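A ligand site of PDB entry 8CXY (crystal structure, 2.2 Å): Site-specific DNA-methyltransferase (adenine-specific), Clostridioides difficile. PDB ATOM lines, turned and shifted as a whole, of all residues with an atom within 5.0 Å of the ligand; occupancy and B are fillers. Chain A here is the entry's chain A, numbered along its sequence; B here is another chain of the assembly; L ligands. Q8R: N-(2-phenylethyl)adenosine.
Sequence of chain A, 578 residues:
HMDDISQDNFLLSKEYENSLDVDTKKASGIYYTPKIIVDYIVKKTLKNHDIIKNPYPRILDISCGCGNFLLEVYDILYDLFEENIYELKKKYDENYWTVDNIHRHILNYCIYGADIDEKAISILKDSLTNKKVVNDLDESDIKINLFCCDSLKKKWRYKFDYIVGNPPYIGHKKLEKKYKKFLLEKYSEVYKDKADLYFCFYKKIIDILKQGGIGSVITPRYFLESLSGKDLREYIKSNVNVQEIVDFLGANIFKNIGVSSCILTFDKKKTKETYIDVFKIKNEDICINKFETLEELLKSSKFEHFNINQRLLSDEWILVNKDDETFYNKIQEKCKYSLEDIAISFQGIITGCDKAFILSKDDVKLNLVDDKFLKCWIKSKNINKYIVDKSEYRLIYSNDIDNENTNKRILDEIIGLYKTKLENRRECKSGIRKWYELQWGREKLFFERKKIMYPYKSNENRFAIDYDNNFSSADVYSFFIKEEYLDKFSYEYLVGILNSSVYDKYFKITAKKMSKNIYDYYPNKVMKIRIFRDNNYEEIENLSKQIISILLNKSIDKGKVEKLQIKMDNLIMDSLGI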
ATOM      1  N   GLY A  29     -16.789  -5.319 -31.393  1.00  0.00           N
ATOM      2  CA  GLY A  29     -17.146  -5.508 -30.004  1.00  0.00           C
ATOM      3  C   GLY A  29     -16.406  -4.581 -29.047  1.00  0.00           C
ATOM      4  O   GLY A  29     -16.780  -4.467 -27.877  1.00  0.00           O
ATOM      5  N   ILE A  30     -15.375  -3.914 -29.552  1.00  0.00           N
ATOM      6  CA  ILE A  30     -14.552  -2.999 -28.770  1.00  0.00           C
ATOM      7  C   ILE A  30     -14.647  -1.607 -29.394  1.00  0.00           C
ATOM      8  O   ILE A  30     -14.421  -1.447 -30.592  1.00  0.00           O
ATOM      9  CB  ILE A  30     -13.085  -3.464 -28.704  1.00  0.00           C
ATOM     10  N   TYR A  31     -14.970  -0.615 -28.562  1.00  0.00           N
ATOM     11  CA  TYR A  31     -15.163   0.771 -29.007  1.00  0.00           C
ATOM     12  C   TYR A  31     -14.154   1.681 -28.322  1.00  0.00           C
ATOM     13  O   TYR A  31     -13.896   1.554 -27.121  1.00  0.00           O
ATOM     14  CB  TYR A  31     -16.589   1.245 -28.694  1.00  0.00           C
ATOM     15  CG  TYR A  31     -17.688   0.382 -29.293  1.00  0.00           C
ATOM     16  CD1 TYR A  31     -18.139  -0.758 -28.626  1.00  0.00           C
ATOM     17  CD2 TYR A  31     -18.254   0.704 -30.510  1.00  0.00           C
ATOM     18  CE1 TYR A  31     -19.134  -1.551 -29.176  1.00  0.00           C
ATOM     19  CE2 TYR A  31     -19.255  -0.095 -31.064  1.00  0.00           C
ATOM     20  CZ  TYR A  31     -19.687  -1.224 -30.395  1.00  0.00           C
ATOM     21  OH  TYR A  31     -20.680  -2.002 -30.946  1.00  0.00           O
ATOM     22  N   ILE A  62     -14.903  -1.123 -15.064  1.00  0.00           N
ATOM     23  CA  ILE A  62     -15.465  -2.471 -15.161  1.00  0.00           C
ATOM     24  C   ILE A  62     -15.744  -2.900 -16.597  1.00  0.00           C
ATOM     25  O   ILE A  62     -16.292  -3.988 -16.797  1.00  0.00           O
ATOM     26  CB  ILE A  62     -16.774  -2.617 -14.362  1.00  0.00           C
ATOM     27  CG1 ILE A  62     -17.828  -1.612 -14.822  1.00  0.00           C
ATOM     28  CG2 ILE A  62     -16.530  -2.445 -12.889  1.00  0.00           C
ATOM     29  CD1 ILE A  62     -19.132  -1.802 -14.096  1.00  0.00           C
ATOM     30  N   SER A  63     -15.425  -2.067 -17.584  1.00  0.00           N
ATOM     31  CA  SER A  63     -15.413  -2.472 -18.983  1.00  0.00           C
ATOM     32  C   SER A  63     -14.173  -1.874 -19.648  1.00  0.00           C
ATOM     33  O   SER A  63     -14.248  -1.196 -20.677  1.00  0.00           O
ATOM     34  CB  SER A  63     -16.709  -2.083 -19.707  1.00  0.00           C
ATOM     35  OG  SER A  63     -17.023  -0.716 -19.524  1.00  0.00           O
ATOM     36  N   GLY A  65     -11.646  -2.726 -21.363  1.00  0.00           N
ATOM     37  CA  GLY A  65     -11.159  -2.999 -22.701  1.00  0.00           C
ATOM     38  C   GLY A  65      -9.636  -3.057 -22.726  1.00  0.00           C
ATOM     39  O   GLY A  65      -9.008  -3.739 -21.906  1.00  0.00           O
ATOM     40  N   ALA A 114     -11.732  -4.562 -15.273  1.00  0.00           N
ATOM     41  CA  ALA A 114     -12.424  -5.809 -15.604  1.00  0.00           C
ATOM     42  C   ALA A 114     -12.965  -5.710 -17.025  1.00  0.00           C
ATOM     43  O   ALA A 114     -13.461  -4.662 -17.435  1.00  0.00           O
ATOM     44  CB  ALA A 114     -13.572  -6.103 -14.630  1.00  0.00           C
ATOM     45  N   ASP A 115     -12.877  -6.820 -17.755  1.00  0.00           N
ATOM     46  CA  ASP A 115     -13.477  -6.877 -19.085  1.00  0.00           C
ATOM     47  C   ASP A 115     -13.716  -8.334 -19.449  1.00  0.00           C
ATOM     48  O   ASP A 115     -12.972  -9.226 -19.034  1.00  0.00           O
ATOM     49  CB  ASP A 115     -12.608  -6.183 -20.136  1.00  0.00           C
ATOM     50  CG  ASP A 115     -13.388  -5.823 -21.384  1.00  0.00           C
ATOM     51  OD1 ASP A 115     -13.837  -6.749 -22.091  1.00  0.00           O
ATOM     52  OD2 ASP A 115     -13.578  -4.614 -21.652  1.00  0.00           O
ATOM     53  N   ILE A 116     -14.775  -8.560 -20.225  1.00  0.00           N
ATOM     54  CA  ILE A 116     -15.139  -9.919 -20.625  1.00  0.00           C
ATOM     55  C   ILE A 116     -14.167 -10.468 -21.668  1.00  0.00           C
ATOM     56  O   ILE A 116     -14.067 -11.684 -21.830  1.00  0.00           O
ATOM     57  CB  ILE A 116     -16.593  -9.942 -21.142  1.00  0.00           C
ATOM     58  CG1 ILE A 116     -17.150 -11.362 -21.159  1.00  0.00           C
ATOM     59  CG2 ILE A 116     -16.686  -9.316 -22.534  1.00  0.00           C
ATOM     60  CD1 ILE A 116     -17.486 -11.892 -19.788  1.00  0.00           C
ATOM     61  N   ASP A 117     -13.442  -9.595 -22.366  1.00  0.00           N
ATOM     62  CA  ASP A 117     -12.572 -10.002 -23.475  1.00  0.00           C
ATOM     63  C   ASP A 117     -11.181 -10.327 -22.945  1.00  0.00           C
ATOM     64  O   ASP A 117     -10.486  -9.457 -22.422  1.00  0.00           O
ATOM     65  CB  ASP A 117     -12.513  -8.906 -24.532  1.00  0.00           C
ATOM     66  CG  ASP A 117     -11.574  -9.254 -25.684  1.00  0.00           C
ATOM     67  OD1 ASP A 117     -11.251 -10.449 -25.852  1.00  0.00           O
ATOM     68  OD2 ASP A 117     -11.170  -8.328 -26.410  1.00  0.00           O
ATOM     69  N   CYS A 149     -13.768 -11.298 -16.707  1.00  0.00           N
ATOM     70  CA  CYS A 149     -15.005 -11.780 -16.110  1.00  0.00           C
ATOM     71  C   CYS A 149     -16.163 -10.947 -16.641  1.00  0.00           C
ATOM     72  O   CYS A 149     -15.970  -9.949 -17.342  1.00  0.00           O
ATOM     73  CB  CYS A 149     -14.958 -11.693 -14.590  1.00  0.00           C
ATOM     74  SG  CYS A 149     -15.004  -9.971 -14.000  1.00  0.00           S
ATOM     75  N   ASP A 150     -17.373 -11.377 -16.292  1.00  0.00           N
ATOM     76  CA  ASP A 150     -18.582 -10.600 -16.496  1.00  0.00           C
ATOM     77  C   ASP A 150     -18.766  -9.703 -15.273  1.00  0.00           C
ATOM     78  O   ASP A 150     -19.043 -10.195 -14.171  1.00  0.00           O
ATOM     79  CB  ASP A 150     -19.786 -11.513 -16.707  1.00  0.00           C
ATOM     80  CG  ASP A 150     -21.093 -10.759 -16.907  1.00  0.00           C
ATOM     81  OD1 ASP A 150     -21.114  -9.515 -16.799  1.00  0.00           O
ATOM     82  OD2 ASP A 150     -22.114 -11.430 -17.187  1.00  0.00           O
ATOM     83  N   SER A 151     -18.618  -8.393 -15.458  1.00  0.00           N
ATOM     84  CA  SER A 151     -18.673  -7.471 -14.326  1.00  0.00           C
ATOM     85  C   SER A 151     -20.032  -7.472 -13.641  1.00  0.00           C
ATOM     86  O   SER A 151     -20.127  -7.113 -12.467  1.00  0.00           O
ATOM     87  CB  SER A 151     -18.318  -6.062 -14.771  1.00  0.00           C
ATOM     88  OG  SER A 151     -16.997  -6.026 -15.282  1.00  0.00           O
ATOM     89  N   LEU A 152     -21.098  -7.863 -14.357  1.00  0.00           N
ATOM     90  CA  LEU A 152     -22.423  -7.913 -13.774  1.00  0.00           C
ATOM     91  C   LEU A 152     -22.649  -9.166 -12.932  1.00  0.00           C
ATOM     92  O   LEU A 152     -23.628  -9.216 -12.188  1.00  0.00           O
ATOM     93  CB  LEU A 152     -23.483  -7.826 -14.872  1.00  0.00           C
ATOM     94  CG  LEU A 152     -23.415  -6.564 -15.749  1.00  0.00           C
ATOM     95  CD1 LEU A 152     -24.596  -6.498 -16.705  1.00  0.00           C
ATOM     96  CD2 LEU A 152     -23.348  -5.303 -14.889  1.00  0.00           C
ATOM     97  N   ASN A 166     -16.482   3.433 -20.116  1.00  0.00           N
ATOM     98  CA  ASN A 166     -17.490   3.410 -21.178  1.00  0.00           C
ATOM     99  C   ASN A 166     -18.100   2.016 -21.212  1.00  0.00           C
ATOM    100  O   ASN A 166     -17.476   1.074 -21.723  1.00  0.00           O
ATOM    101  CB  ASN A 166     -16.863   3.778 -22.514  1.00  0.00           C
ATOM    102  CG  ASN A 166     -17.880   3.822 -23.645  1.00  0.00           C
ATOM    103  OD1 ASN A 166     -19.083   3.887 -23.415  1.00  0.00           O
ATOM    104  ND2 ASN A 166     -17.395   3.788 -24.877  1.00  0.00           N
ATOM    105  N   PRO A 167     -19.307   1.833 -20.665  1.00  0.00           N
ATOM    106  CA  PRO A 167     -19.903   0.491 -20.593  1.00  0.00           C
ATOM    107  C   PRO A 167     -20.408   0.040 -21.954  1.00  0.00           C
ATOM    108  O   PRO A 167     -20.537   0.857 -22.880  1.00  0.00           O
ATOM    109  CB  PRO A 167     -21.066   0.687 -19.613  1.00  0.00           C
ATOM    110  CG  PRO A 167     -21.479   2.099 -19.841  1.00  0.00           C
ATOM    111  CD  PRO A 167     -20.184   2.857 -20.087  1.00  0.00           C
ATOM    112  N   PRO A 168     -20.696  -1.248 -22.113  1.00  0.00           N
ATOM    113  CA  PRO A 168     -21.347  -1.705 -23.346  1.00  0.00           C
ATOM    114  C   PRO A 168     -22.797  -1.264 -23.420  1.00  0.00           C
ATOM    115  O   PRO A 168     -23.497  -1.181 -22.411  1.00  0.00           O
ATOM    116  CB  PRO A 168     -21.250  -3.233 -23.251  1.00  0.00           C
ATOM    117  CG  PRO A 168     -21.200  -3.495 -21.782  1.00  0.00           C
ATOM    118  CD  PRO A 168     -20.380  -2.364 -21.215  1.00  0.00           C
ATOM    119  N   ILE A 170     -26.225  -2.422 -25.253  1.00  0.00           N
ATOM    120  CA  ILE A 170     -26.913  -3.466 -26.010  1.00  0.00           C
ATOM    121  C   ILE A 170     -28.404  -3.373 -25.723  1.00  0.00           C
ATOM    122  O   ILE A 170     -28.819  -3.483 -24.560  1.00  0.00           O
ATOM    123  CB  ILE A 170     -26.400  -4.887 -25.674  1.00  0.00           C
ATOM    124  CG1 ILE A 170     -24.865  -4.937 -25.748  1.00  0.00           C
ATOM    125  CG2 ILE A 170     -26.997  -5.884 -26.640  1.00  0.00           C
ATOM    126  CD1 ILE A 170     -24.277  -6.299 -25.508  1.00  0.00           C
ATOM    127  N   LEU A 175     -29.694  -8.309 -27.426  1.00  0.00           N
ATOM    128  CA  LEU A 175     -29.253  -8.974 -26.218  1.00  0.00           C
ATOM    129  C   LEU A 175     -29.776 -10.402 -26.197  1.00  0.00           C
ATOM    130  O   LEU A 175     -30.947 -10.649 -26.510  1.00  0.00           O
ATOM    131  CB  LEU A 175     -29.717  -8.211 -24.967  1.00  0.00           C
ATOM    132  CG  LEU A 175     -29.040  -8.574 -23.652  1.00  0.00           C
ATOM    133  CD1 LEU A 175     -27.531  -8.453 -23.776  1.00  0.00           C
ATOM    134  CD2 LEU A 175     -29.559  -7.680 -22.532  1.00  0.00           C
ATOM    135  N   TYR A 179     -29.408 -14.531 -21.346  1.00  0.00           N
ATOM    136  CA  TYR A 179     -28.803 -13.537 -20.473  1.00  0.00           C
ATOM    137  C   TYR A 179     -29.838 -12.562 -19.934  1.00  0.00           C
ATOM    138  O   TYR A 179     -29.720 -12.111 -18.791  1.00  0.00           O
ATOM    139  CB  TYR A 179     -27.700 -12.773 -21.219  1.00  0.00           C
ATOM    140  CG  TYR A 179     -26.788 -12.001 -20.311  1.00  0.00           C
ATOM    141  CD1 TYR A 179     -25.729 -12.630 -19.651  1.00  0.00           C
ATOM    142  CD2 TYR A 179     -26.961 -10.641 -20.095  1.00  0.00           C
ATOM    143  CE1 TYR A 179     -24.892 -11.935 -18.820  1.00  0.00           C
ATOM    144  CE2 TYR A 179     -26.122  -9.932 -19.265  1.00  0.00           C
ATOM    145  CZ  TYR A 179     -25.091 -10.582 -18.630  1.00  0.00           C
ATOM    146  OH  TYR A 179     -24.264  -9.878 -17.797  1.00  0.00           O
ATOM    147  N   LEU A 197     -28.637  -2.861 -21.738  1.00  0.00           N
ATOM    148  CA  LEU A 197     -27.609  -3.447 -20.884  1.00  0.00           C
ATOM    149  C   LEU A 197     -26.865  -2.384 -20.072  1.00  0.00           C
ATOM    150  O   LEU A 197     -26.484  -2.625 -18.922  1.00  0.00           O
ATOM    151  CB  LEU A 197     -26.634  -4.258 -21.731  1.00  0.00           C
ATOM    152  CG  LEU A 197     -25.446  -4.881 -20.980  1.00  0.00           C
ATOM    153  CD1 LEU A 197     -25.931  -5.948 -20.027  1.00  0.00           C
ATOM    154  CD2 LEU A 197     -24.441  -5.452 -21.968  1.00  0.00           C
ATOM    155  N   PHE A 201     -25.061  -1.551 -15.876  1.00  0.00           N
ATOM    156  CA  PHE A 201     -23.732  -1.070 -15.521  1.00  0.00           C
ATOM    157  C   PHE A 201     -23.823   0.183 -14.649  1.00  0.00           C
ATOM    158  O   PHE A 201     -23.014   0.360 -13.745  1.00  0.00           O
ATOM    159  CB  PHE A 201     -22.920  -0.818 -16.783  1.00  0.00           C
ATOM    160  CG  PHE A 201     -22.261  -2.060 -17.306  1.00  0.00           C
ATOM    161  CD1 PHE A 201     -22.980  -2.997 -18.031  1.00  0.00           C
ATOM    162  CD2 PHE A 201     -20.922  -2.305 -17.056  1.00  0.00           C
ATOM    163  CE1 PHE A 201     -22.380  -4.147 -18.505  1.00  0.00           C
ATOM    164  CE2 PHE A 201     -20.310  -3.451 -17.533  1.00  0.00           C
ATOM    165  CZ  PHE A 201     -21.040  -4.379 -18.257  1.00  0.00           C
ATOM    166  P    DA B   8     -28.939   0.460 -30.978  1.00  0.00           P
ATOM    167  OP1  DA B   8     -28.879  -0.544 -32.058  1.00  0.00           O
ATOM    168  OP2  DA B   8     -29.182   0.035 -29.577  1.00  0.00           O
ATOM    169  O5'  DA B   8     -27.606   1.339 -31.035  1.00  0.00           O
ATOM    170  C5'  DA B   8     -26.521   1.090 -30.168  1.00  0.00           C
ATOM    171  C4'  DA B   8     -25.250   1.639 -30.776  1.00  0.00           C
ATOM    172  O4'  DA B   8     -24.254   1.882 -29.746  1.00  0.00           O
ATOM    173  C3'  DA B   8     -24.579   0.722 -31.787  1.00  0.00           C
ATOM    174  O3'  DA B   8     -24.123   1.501 -32.867  1.00  0.00           O
ATOM    175  C2'  DA B   8     -23.407   0.133 -31.001  1.00  0.00           C
ATOM    176  C1'  DA B   8     -23.025   1.325 -30.147  1.00  0.00           C
ATOM    177  N9   DA B   8     -22.269   0.985 -28.944  1.00  0.00           N
ATOM    178  C8   DA B   8     -22.447  -0.098 -28.134  1.00  0.00           C
ATOM    179  N7   DA B   8     -21.628  -0.141 -27.110  1.00  0.00           N
ATOM    180  C5   DA B   8     -20.853   1.001 -27.257  1.00  0.00           C
ATOM    181  C6   DA B   8     -19.798   1.556 -26.487  1.00  0.00           C
ATOM    182  N6   DA B   8     -19.333   0.979 -25.377  1.00  0.00           N
ATOM    183  N1   DA B   8     -19.249   2.714 -26.907  1.00  0.00           N
ATOM    184  C2   DA B   8     -19.728   3.286 -28.015  1.00  0.00           C
ATOM    185  N3   DA B   8     -20.714   2.869 -28.817  1.00  0.00           N
ATOM    186  C4   DA B   8     -21.236   1.709 -28.383  1.00  0.00           C
HETATM  187  C12 Q8R L   1     -22.454  -9.912 -21.827  1.00  0.00           C
HETATM  188  O1  Q8R L   1     -15.441  -6.491 -23.935  1.00  0.00           O
HETATM  189  C13 Q8R L   1     -22.563  -9.085 -22.927  1.00  0.00           C
HETATM  190  C14 Q8R L   1     -23.466  -9.360 -23.939  1.00  0.00           C
HETATM  191  C15 Q8R L   1     -24.271 -10.475 -23.860  1.00  0.00           C
HETATM  192  C16 Q8R L   1     -24.173 -11.315 -22.769  1.00  0.00           C
HETATM  193  C17 Q8R L   1     -23.270 -11.041 -21.757  1.00  0.00           C
HETATM  194  O2  Q8R L   1     -16.834  -1.150 -25.107  1.00  0.00           O
HETATM  195  O3  Q8R L   1     -17.174  -3.711 -22.570  1.00  0.00           O
HETATM  196  O   Q8R L   1     -14.332  -4.049 -24.112  1.00  0.00           O
HETATM  197  C7  Q8R L   1     -17.918  -6.316 -20.673  1.00  0.00           C
HETATM  198  C8  Q8R L   1     -17.434  -6.751 -18.557  1.00  0.00           C
HETATM  199  C9  Q8R L   1     -19.505  -7.440 -19.297  1.00  0.00           C
HETATM  200  C10 Q8R L   1     -21.727  -8.315 -20.006  1.00  0.00           C
HETATM  201  C11 Q8R L   1     -21.455  -9.627 -20.731  1.00  0.00           C
HETATM  202  N4  Q8R L   1     -20.675  -8.063 -19.038  1.00  0.00           N
HETATM  203  N   Q8R L   1     -17.833  -5.853 -21.955  1.00  0.00           N
HETATM  204  C   Q8R L   1     -15.716  -4.111 -24.414  1.00  0.00           C
HETATM  205  N1  Q8R L   1     -19.842  -6.843 -21.779  1.00  0.00           N
HETATM  206  C1  Q8R L   1     -16.361  -5.410 -23.947  1.00  0.00           C
HETATM  207  N2  Q8R L   1     -17.007  -6.211 -19.702  1.00  0.00           N
HETATM  208  C2  Q8R L   1     -16.481  -3.033 -23.641  1.00  0.00           C
HETATM  209  C3  Q8R L   1     -17.482  -2.231 -24.456  1.00  0.00           C
HETATM  210  C4  Q8R L   1     -16.751  -5.055 -22.524  1.00  0.00           C
HETATM  211  C5  Q8R L   1     -19.001  -6.214 -22.564  1.00  0.00           C
HETATM  212  C6  Q8R L   1     -19.172  -6.914 -20.567  1.00  0.00           C
HETATM  213  N3  Q8R L   1     -18.606  -7.353 -18.306  1.00  0.00           N
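A nitrogen (N4) of the ligand is in hydrogen-bond range of the side-chain carboxylate (OD1) of Asp 150 (2.7 Å). N6 of DA 8 of chain B sits at hydrogen-bond distance from O2 of the ligand (3.3 Å). N of Ser 151 is in hydrogen-bond range of N3 of the ligand (3.0 Å). The backbone NH of Ile 116 lies within hydrogen-bond range of a nitrogen (N2) of the ligand (3.3 Å). The side-chain carboxylate (OD1) of Asp 115 sits at hydrogen-bond distance from an oxygen (O1) of the ligand.
The side-chain carboxylate of Asp 150 sits at hydrogen-bond distance from the backbone NH of Leu 152. The side-chain hydroxyl of Ser 151 lies within hydrogen-bond range of the backbone carbonyl oxygen of Ile 62. N1 of DA 8 of chain B lies within hydrogen-bond range of the side-chain amide nitrogen (ND2) of Asn 166 (3.0 Å). The side-chain carboxylate (OD1) of Asp 115 lies within hydrogen-bond range of the backbone NH (N) of Asp 117 (2.9 Å). The backbone carbonyl oxygen (O) of Ile 170 lies within hydrogen-bond range of the backbone NH (N) of Leu 197. The backbone NH (N) of Cys 149 is in hydrogen-bond range of the backbone carbonyl oxygen (O) of Asp 115 (3.2 Å). OG of Ser 63 is in hydrogen-bond range of O of Asn 166, 2.9 Å away. OD2 of Asp 115 is in hydrogen-bond range of N of Gly 65, 2.7 Å away.
Merely in contact with the ligand: Ser 63 (3.3 Å), Ile 62 (3.5 Å), Tyr 179 (3.5 Å), Ile 170 (3.5 Å), Phe 201 (3.6 Å), Pro 168 (3.6 Å), Gly 65 (3.6 Å), Gly 29 (3.6 Å), Cys 149 (3.7 Å), Tyr 31 (3.8 Å), Leu 175 (3.8 Å) and Asp 117 (3.8 Å). Hydrophobic or aromatic side chains that line the ligand: Tyr 31, Ile 116, Pro 168, Ile 170, Leu 175, Tyr 179 and Phe 201. Of the 23 residues printed, 17 come within 4 Å of the ligand. Along chain A the residues within 4 Å of the ligand span positions 29 to 201. The nearest printed residue that does not touch the ligand is Asn 166 (4.1 Å).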
